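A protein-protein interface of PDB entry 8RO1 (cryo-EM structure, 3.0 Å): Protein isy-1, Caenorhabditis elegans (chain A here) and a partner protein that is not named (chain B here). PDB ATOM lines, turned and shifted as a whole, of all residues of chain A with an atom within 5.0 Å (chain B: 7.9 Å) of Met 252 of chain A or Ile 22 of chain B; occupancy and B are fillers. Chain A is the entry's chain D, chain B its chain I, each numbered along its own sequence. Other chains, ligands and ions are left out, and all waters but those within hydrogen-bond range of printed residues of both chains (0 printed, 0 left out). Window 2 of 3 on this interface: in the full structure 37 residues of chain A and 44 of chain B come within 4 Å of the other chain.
The side-chain sulfur (SD) of Met 252 of chain A lies within hydrogen-bond range of the backbone NH (N) of Gly 21 of chain B (3.1 Å).
The side-chain amino group (NZ) of Lys 20 of chain B sits at hydrogen-bond distance from the side-chain sulfur (SD) of Met 19 of chain B, 3.7 Å away. The side-chain carboxylate (OE1) of Glu 30 of chain B sits at hydrogen-bond distance from the side-chain hydroxyl (OH) of Tyr 46 of chain B (2.6 Å). OE2 of Glu 30 of chain B is in salt-bridge range of NH1 of Arg 66 of chain B, 2.6 Å away.
Ile 22 of chain B touches just these residues of chain A: Ile 249 (3.8 Å) and Met 252 (3.7 Å). No residue of chain B comes within 4 Å of Glu 251 of chain A. Of the printed residues of chain B, Leu 253 of chain A touches Glu 30. Printed residues of chain A within 4 Å of Arg 66 of chain B: Ile 249 (3.4 Å). The nearest residue of chain A that does not touch Ile 22 of chain B is Leu 253 of chain A (4.02 Å). The nearest printed residue of chain A that does not touch Arg 66 of chain B is Glu 250 of chain A (6.5 Å).
Among the printed residues, merely in contact across the chains: Ile 249 of chain A with Ile 22 of chain B, Ile 249 of chain A with Glu 30 of chain B, Ile 249 of chain A with Arg 66 of chain B, Met 252 of chain A with Lys 20 of chain B, Met 252 of chain A with Ile 22 of chain B and Leu 253 of chain A with Glu 30 of chain B.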
ATOM      1  N   ASP A 248      31.635 -16.849  23.358  1.00  0.00           N
ATOM      2  CA  ASP A 248      31.838 -16.038  22.160  1.00  0.00           C
ATOM      3  C   ASP A 248      31.166 -16.660  20.942  1.00  0.00           C
ATOM      4  O   ASP A 248      30.653 -15.940  20.079  1.00  0.00           O
ATOM      5  CB  ASP A 248      33.330 -15.837  21.897  1.00  0.00           C
ATOM      6  CG  ASP A 248      34.057 -15.267  23.091  1.00  0.00           C
ATOM      7  OD1 ASP A 248      33.956 -14.043  23.315  1.00  0.00           O
ATOM      8  OD2 ASP A 248      34.729 -16.038  23.805  1.00  0.00           O
ATOM      9  N   ILE A 249      31.195 -17.987  20.828  1.00  0.00           N
ATOM     10  CA  ILE A 249      30.563 -18.628  19.680  1.00  0.00           C
ATOM     11  C   ILE A 249      29.047 -18.661  19.845  1.00  0.00           C
ATOM     12  O   ILE A 249      28.317 -18.728  18.849  1.00  0.00           O
ATOM     13  CB  ILE A 249      31.146 -20.035  19.449  1.00  0.00           C
ATOM     14  CG1 ILE A 249      30.832 -20.520  18.027  1.00  0.00           C
ATOM     15  CG2 ILE A 249      30.626 -21.031  20.467  1.00  0.00           C
ATOM     16  CD1 ILE A 249      31.684 -21.680  17.577  1.00  0.00           C
ATOM     17  N   GLU A 250      28.549 -18.631  21.086  1.00  0.00           N
ATOM     18  CA  GLU A 250      27.108 -18.529  21.302  1.00  0.00           C
ATOM     19  C   GLU A 250      26.551 -17.226  20.738  1.00  0.00           C
ATOM     20  O   GLU A 250      25.504 -17.229  20.080  1.00  0.00           O
ATOM     21  CB  GLU A 250      26.790 -18.662  22.792  1.00  0.00           C
ATOM     22  CG  GLU A 250      25.300 -18.809  23.106  1.00  0.00           C
ATOM     23  CD  GLU A 250      24.594 -17.504  23.447  1.00  0.00           C
ATOM     24  OE1 GLU A 250      25.253 -16.522  23.854  1.00  0.00           O
ATOM     25  OE2 GLU A 250      23.353 -17.466  23.309  1.00  0.00           O
ATOM     26  N   GLU A 251      27.228 -16.104  20.979  1.00  0.00           N
ATOM     27  CA  GLU A 251      26.734 -14.839  20.442  1.00  0.00           C
ATOM     28  C   GLU A 251      27.051 -14.698  18.958  1.00  0.00           C
ATOM     29  O   GLU A 251      26.359 -13.959  18.251  1.00  0.00           O
ATOM     30  CB  GLU A 251      27.309 -13.634  21.197  1.00  0.00           C
ATOM     31  CG  GLU A 251      28.841 -13.518  21.263  1.00  0.00           C
ATOM     32  CD  GLU A 251      29.465 -12.820  20.053  1.00  0.00           C
ATOM     33  OE1 GLU A 251      28.750 -12.114  19.311  1.00  0.00           O
ATOM     34  OE2 GLU A 251      30.684 -12.989  19.840  1.00  0.00           O
ATOM     35  N   MET A 252      28.092 -15.383  18.474  1.00  0.00           N
ATOM     36  CA  MET A 252      28.418 -15.343  17.052  1.00  0.00           C
ATOM     37  C   MET A 252      27.340 -16.026  16.216  1.00  0.00           C
ATOM     38  O   MET A 252      26.890 -15.479  15.203  1.00  0.00           O
ATOM     39  CB  MET A 252      29.785 -16.000  16.816  1.00  0.00           C
ATOM     40  CG  MET A 252      30.324 -15.939  15.372  1.00  0.00           C
ATOM     41  SD  MET A 252      31.676 -17.092  15.033  1.00  0.00           S
ATOM     42  CE  MET A 252      32.791 -16.788  16.398  1.00  0.00           C
ATOM     43  N   LEU A 253      26.910 -17.222  16.618  1.00  0.00           N
ATOM     44  CA  LEU A 253      25.792 -17.859  15.933  1.00  0.00           C
ATOM     45  C   LEU A 253      24.475 -17.138  16.173  1.00  0.00           C
ATOM     46  O   LEU A 253      23.565 -17.252  15.345  1.00  0.00           O
ATOM     47  CB  LEU A 253      25.689 -19.328  16.358  1.00  0.00           C
ATOM     48  CG  LEU A 253      25.140 -19.730  17.734  1.00  0.00           C
ATOM     49  CD1 LEU A 253      23.625 -19.955  17.736  1.00  0.00           C
ATOM     50  CD2 LEU A 253      25.856 -20.965  18.250  1.00  0.00           C
ATOM     51  N   LEU A 254      24.356 -16.389  17.271  1.00  0.00           N
ATOM     52  CA  LEU A 254      23.139 -15.622  17.523  1.00  0.00           C
ATOM     53  C   LEU A 254      22.949 -14.540  16.470  1.00  0.00           C
ATOM     54  O   LEU A 254      21.871 -14.415  15.879  1.00  0.00           O
ATOM     55  CB  LEU A 254      23.190 -15.009  18.923  1.00  0.00           C
ATOM     56  CG  LEU A 254      22.113 -13.993  19.333  1.00  0.00           C
ATOM     57  CD1 LEU A 254      20.705 -14.542  19.130  1.00  0.00           C
ATOM     58  CD2 LEU A 254      22.326 -13.578  20.783  1.00  0.00           C
ATOM     59  N   GLU A 255      23.995 -13.753  16.218  1.00  0.00           N
ATOM     60  CA  GLU A 255      23.926 -12.714  15.195  1.00  0.00           C
ATOM     61  C   GLU A 255      23.675 -13.301  13.813  1.00  0.00           C
ATOM     62  O   GLU A 255      22.963 -12.704  13.000  1.00  0.00           O
ATOM     63  CB  GLU A 255      25.219 -11.902  15.198  1.00  0.00           C
ATOM     64  CG  GLU A 255      25.342 -10.961  16.403  1.00  0.00           C
ATOM     65  CD  GLU A 255      26.669 -11.048  17.156  1.00  0.00           C
ATOM     66  OE1 GLU A 255      27.654 -11.620  16.640  1.00  0.00           O
ATOM     67  OE2 GLU A 255      26.721 -10.539  18.296  1.00  0.00           O
ATOM     68  N   GLN A 256      24.252 -14.465  13.526  1.00  0.00           N
ATOM     69  CA  GLN A 256      24.052 -15.082  12.219  1.00  0.00           C
ATOM     70  C   GLN A 256      22.592 -15.485  12.018  1.00  0.00           C
ATOM     71  O   GLN A 256      22.002 -15.208  10.966  1.00  0.00           O
ATOM     72  CB  GLN A 256      24.982 -16.289  12.074  1.00  0.00           C
ATOM     73  CG  GLN A 256      24.979 -16.962  10.697  1.00  0.00           C
ATOM     74  CD  GLN A 256      25.640 -16.100   9.638  1.00  0.00           C
ATOM     75  OE1 GLN A 256      26.488 -15.260   9.943  1.00  0.00           O
ATOM     76  NE2 GLN A 256      25.253 -16.304   8.383  1.00  0.00           N
ATOM     77  N   MET B  19      38.717 -14.601  12.847  1.00  0.00           N
ATOM     78  CA  MET B  19      38.528 -15.613  13.881  1.00  0.00           C
ATOM     79  C   MET B  19      37.081 -16.070  14.034  1.00  0.00           C
ATOM     80  O   MET B  19      36.831 -16.979  14.835  1.00  0.00           O
ATOM     81  CB  MET B  19      39.068 -15.103  15.233  1.00  0.00           C
ATOM     82  CG  MET B  19      38.537 -13.749  15.777  1.00  0.00           C
ATOM     83  SD  MET B  19      36.798 -13.641  16.264  1.00  0.00           S
ATOM     84  CE  MET B  19      36.756 -14.765  17.657  1.00  0.00           C
ATOM     85  N   LYS B  20      36.136 -15.485  13.293  1.00  0.00           N
ATOM     86  CA  LYS B  20      34.713 -15.764  13.437  1.00  0.00           C
ATOM     87  C   LYS B  20      34.136 -16.291  12.131  1.00  0.00           C
ATOM     88  O   LYS B  20      34.587 -15.931  11.040  1.00  0.00           O
ATOM     89  CB  LYS B  20      33.947 -14.503  13.875  1.00  0.00           C
ATOM     90  CG  LYS B  20      34.219 -13.257  13.021  1.00  0.00           C
ATOM     91  CD  LYS B  20      33.260 -12.083  13.299  1.00  0.00           C
ATOM     92  CE  LYS B  20      33.179 -11.650  14.769  1.00  0.00           C
ATOM     93  NZ  LYS B  20      34.440 -11.021  15.246  1.00  0.00           N
ATOM     94  N   GLY B  21      33.134 -17.158  12.258  1.00  0.00           N
ATOM     95  CA  GLY B  21      32.454 -17.714  11.106  1.00  0.00           C
ATOM     96  C   GLY B  21      31.610 -18.925  11.443  1.00  0.00           C
ATOM     97  O   GLY B  21      32.096 -19.885  12.050  1.00  0.00           O
ATOM     98  N   ILE B  22      30.339 -18.881  11.051  1.00  0.00           N
ATOM     99  CA  ILE B  22      29.364 -19.931  11.317  1.00  0.00           C
ATOM    100  C   ILE B  22      28.745 -20.335   9.988  1.00  0.00           C
ATOM    101  O   ILE B  22      28.507 -19.486   9.122  1.00  0.00           O
ATOM    102  CB  ILE B  22      28.283 -19.473  12.324  1.00  0.00           C
ATOM    103  CG1 ILE B  22      28.894 -19.146  13.692  1.00  0.00           C
ATOM    104  CG2 ILE B  22      27.189 -20.514  12.488  1.00  0.00           C
ATOM    105  CD1 ILE B  22      29.473 -20.336  14.470  1.00  0.00           C
ATOM    106  N   SER B  23      28.478 -21.625   9.830  1.00  0.00           N
ATOM    107  CA  SER B  23      27.915 -22.129   8.588  1.00  0.00           C
ATOM    108  C   SER B  23      26.423 -21.807   8.548  1.00  0.00           C
ATOM    109  O   SER B  23      25.900 -21.056   9.376  1.00  0.00           O
ATOM    110  CB  SER B  23      28.164 -23.626   8.460  1.00  0.00           C
ATOM    111  OG  SER B  23      27.208 -24.350   9.212  1.00  0.00           O
ATOM    112  N   SER B  24      25.722 -22.386   7.575  1.00  0.00           N
ATOM    113  CA  SER B  24      24.265 -22.407   7.530  1.00  0.00           C
ATOM    114  C   SER B  24      23.674 -23.761   7.896  1.00  0.00           C
ATOM    115  O   SER B  24      22.446 -23.895   7.903  1.00  0.00           O
ATOM    116  CB  SER B  24      23.780 -21.997   6.134  1.00  0.00           C
ATOM    117  OG  SER B  24      24.053 -23.005   5.176  1.00  0.00           O
ATOM    118  N   GLU B  25      24.504 -24.753   8.233  1.00  0.00           N
ATOM    119  CA  GLU B  25      24.116 -26.159   8.141  1.00  0.00           C
ATOM    120  C   GLU B  25      24.462 -26.932   9.410  1.00  0.00           C
ATOM    121  O   GLU B  25      23.816 -27.944   9.696  1.00  0.00           O
ATOM    122  CB  GLU B  25      24.773 -26.815   6.918  1.00  0.00           C
ATOM    123  CG  GLU B  25      26.304 -26.774   6.882  1.00  0.00           C
ATOM    124  CD  GLU B  25      26.839 -25.762   5.883  1.00  0.00           C
ATOM    125  OE1 GLU B  25      26.341 -24.617   5.858  1.00  0.00           O
ATOM    126  OE2 GLU B  25      27.762 -26.117   5.121  1.00  0.00           O
ATOM    127  N   ASP B  26      25.467 -26.478  10.172  1.00  0.00           N
ATOM    128  CA  ASP B  26      25.830 -27.091  11.449  1.00  0.00           C
ATOM    129  C   ASP B  26      25.471 -26.212  12.651  1.00  0.00           C
ATOM    130  O   ASP B  26      25.795 -26.575  13.785  1.00  0.00           O
ATOM    131  CB  ASP B  26      27.328 -27.453  11.461  1.00  0.00           C
ATOM    132  CG  ASP B  26      28.259 -26.254  11.253  1.00  0.00           C
ATOM    133  OD1 ASP B  26      27.830 -25.088  11.368  1.00  0.00           O
ATOM    134  OD2 ASP B  26      29.450 -26.488  10.960  1.00  0.00           O
ATOM    135  N   VAL B  27      24.844 -25.059  12.426  1.00  0.00           N
ATOM    136  CA  VAL B  27      24.298 -24.189  13.475  1.00  0.00           C
ATOM    137  C   VAL B  27      23.357 -24.938  14.419  1.00  0.00           C
ATOM    138  O   VAL B  27      23.383 -24.659  15.625  1.00  0.00           O
ATOM    139  CB  VAL B  27      23.582 -22.936  12.917  1.00  0.00           C
ATOM    140  CG1 VAL B  27      23.457 -21.876  14.014  1.00  0.00           C
ATOM    141  CG2 VAL B  27      24.311 -22.309  11.703  1.00  0.00           C
ATOM    142  N   PRO B  28      22.486 -25.848  13.946  1.00  0.00           N
ATOM    143  CA  PRO B  28      21.678 -26.622  14.907  1.00  0.00           C
ATOM    144  C   PRO B  28      22.474 -27.448  15.897  1.00  0.00           C
ATOM    145  O   PRO B  28      22.063 -27.556  17.057  1.00  0.00           O
ATOM    146  CB  PRO B  28      20.838 -27.524  13.995  1.00  0.00           C
ATOM    147  CG  PRO B  28      20.684 -26.756  12.773  1.00  0.00           C
ATOM    148  CD  PRO B  28      21.996 -26.069  12.570  1.00  0.00           C
ATOM    149  N   GLU B  30      25.584 -26.677  16.949  1.00  0.00           N
ATOM    150  CA  GLU B  30      26.223 -25.710  17.835  1.00  0.00           C
ATOM    151  C   GLU B  30      25.239 -25.162  18.858  1.00  0.00           C
ATOM    152  O   GLU B  30      25.548 -25.082  20.052  1.00  0.00           O
ATOM    153  CB  GLU B  30      26.807 -24.571  16.995  1.00  0.00           C
ATOM    154  CG  GLU B  30      27.845 -23.714  17.686  1.00  0.00           C
ATOM    155  CD  GLU B  30      29.135 -24.452  17.949  1.00  0.00           C
ATOM    156  OE1 GLU B  30      30.018 -24.462  17.064  1.00  0.00           O
ATOM    157  OE2 GLU B  30      29.266 -25.031  19.045  1.00  0.00           O
ATOM    158  N   TYR B  46      27.794 -33.470  16.945  1.00  0.00           N
ATOM    159  CA  TYR B  46      28.380 -32.376  16.186  1.00  0.00           C
ATOM    160  C   TYR B  46      29.602 -32.864  15.420  1.00  0.00           C
ATOM    161  O   TYR B  46      29.720 -32.645  14.210  1.00  0.00           O
ATOM    162  CB  TYR B  46      28.730 -31.245  17.153  1.00  0.00           C
ATOM    163  CG  TYR B  46      29.146 -29.906  16.584  1.00  0.00           C
ATOM    164  CD1 TYR B  46      28.830 -29.525  15.292  1.00  0.00           C
ATOM    165  CD2 TYR B  46      29.833 -29.004  17.373  1.00  0.00           C
ATOM    166  CE1 TYR B  46      29.211 -28.304  14.806  1.00  0.00           C
ATOM    167  CE2 TYR B  46      30.206 -27.784  16.899  1.00  0.00           C
ATOM    168  CZ  TYR B  46      29.891 -27.431  15.618  1.00  0.00           C
ATOM    169  OH  TYR B  46      30.265 -26.195  15.145  1.00  0.00           O
ATOM    170  N   LYS B  50      30.147 -33.204  11.421  1.00  0.00           N
ATOM    171  CA  LYS B  50      31.177 -32.456  10.718  1.00  0.00           C
ATOM    172  C   LYS B  50      32.075 -33.350   9.873  1.00  0.00           C
ATOM    173  O   LYS B  50      32.600 -32.894   8.853  1.00  0.00           O
ATOM    174  CB  LYS B  50      32.007 -31.667  11.721  1.00  0.00           C
ATOM    175  CG  LYS B  50      32.698 -30.486  11.111  1.00  0.00           C
ATOM    176  CD  LYS B  50      31.773 -29.291  11.019  1.00  0.00           C
ATOM    177  CE  LYS B  50      32.443 -28.150  10.285  1.00  0.00           C
ATOM    178  NZ  LYS B  50      31.631 -26.916  10.351  1.00  0.00           N
ATOM    179  N   LEU B  62      39.481 -27.529  16.250  1.00  0.00           N
ATOM    180  CA  LEU B  62      38.786 -26.542  17.064  1.00  0.00           C
ATOM    181  C   LEU B  62      37.634 -27.173  17.837  1.00  0.00           C
ATOM    182  O   LEU B  62      37.502 -26.961  19.045  1.00  0.00           O
ATOM    183  CB  LEU B  62      38.293 -25.412  16.163  1.00  0.00           C
ATOM    184  CG  LEU B  62      37.468 -24.284  16.770  1.00  0.00           C
ATOM    185  CD1 LEU B  62      38.329 -23.547  17.788  1.00  0.00           C
ATOM    186  CD2 LEU B  62      36.954 -23.351  15.688  1.00  0.00           C
ATOM    187  N   ARG B  66      37.483 -27.497  21.843  1.00  0.00           N
ATOM    188  CA  ARG B  66      36.340 -26.932  22.547  1.00  0.00           C
ATOM    189  C   ARG B  66      35.619 -27.966  23.406  1.00  0.00           C
ATOM    190  O   ARG B  66      35.292 -27.701  24.566  1.00  0.00           O
ATOM    191  CB  ARG B  66      35.392 -26.319  21.532  1.00  0.00           C
ATOM    192  CG  ARG B  66      35.910 -25.019  20.962  1.00  0.00           C
ATOM    193  CD  ARG B  66      35.024 -24.499  19.873  1.00  0.00           C
ATOM    194  NE  ARG B  66      33.683 -24.266  20.388  1.00  0.00           N
ATOM    195  CZ  ARG B  66      32.548 -24.540  19.762  1.00  0.00           C
ATOM    196  NH1 ARG B  66      31.409 -24.454  20.437  1.00  0.00           N
ATOM    197  NH2 ARG B  66      32.513 -24.858  18.478  1.00  0.00           N
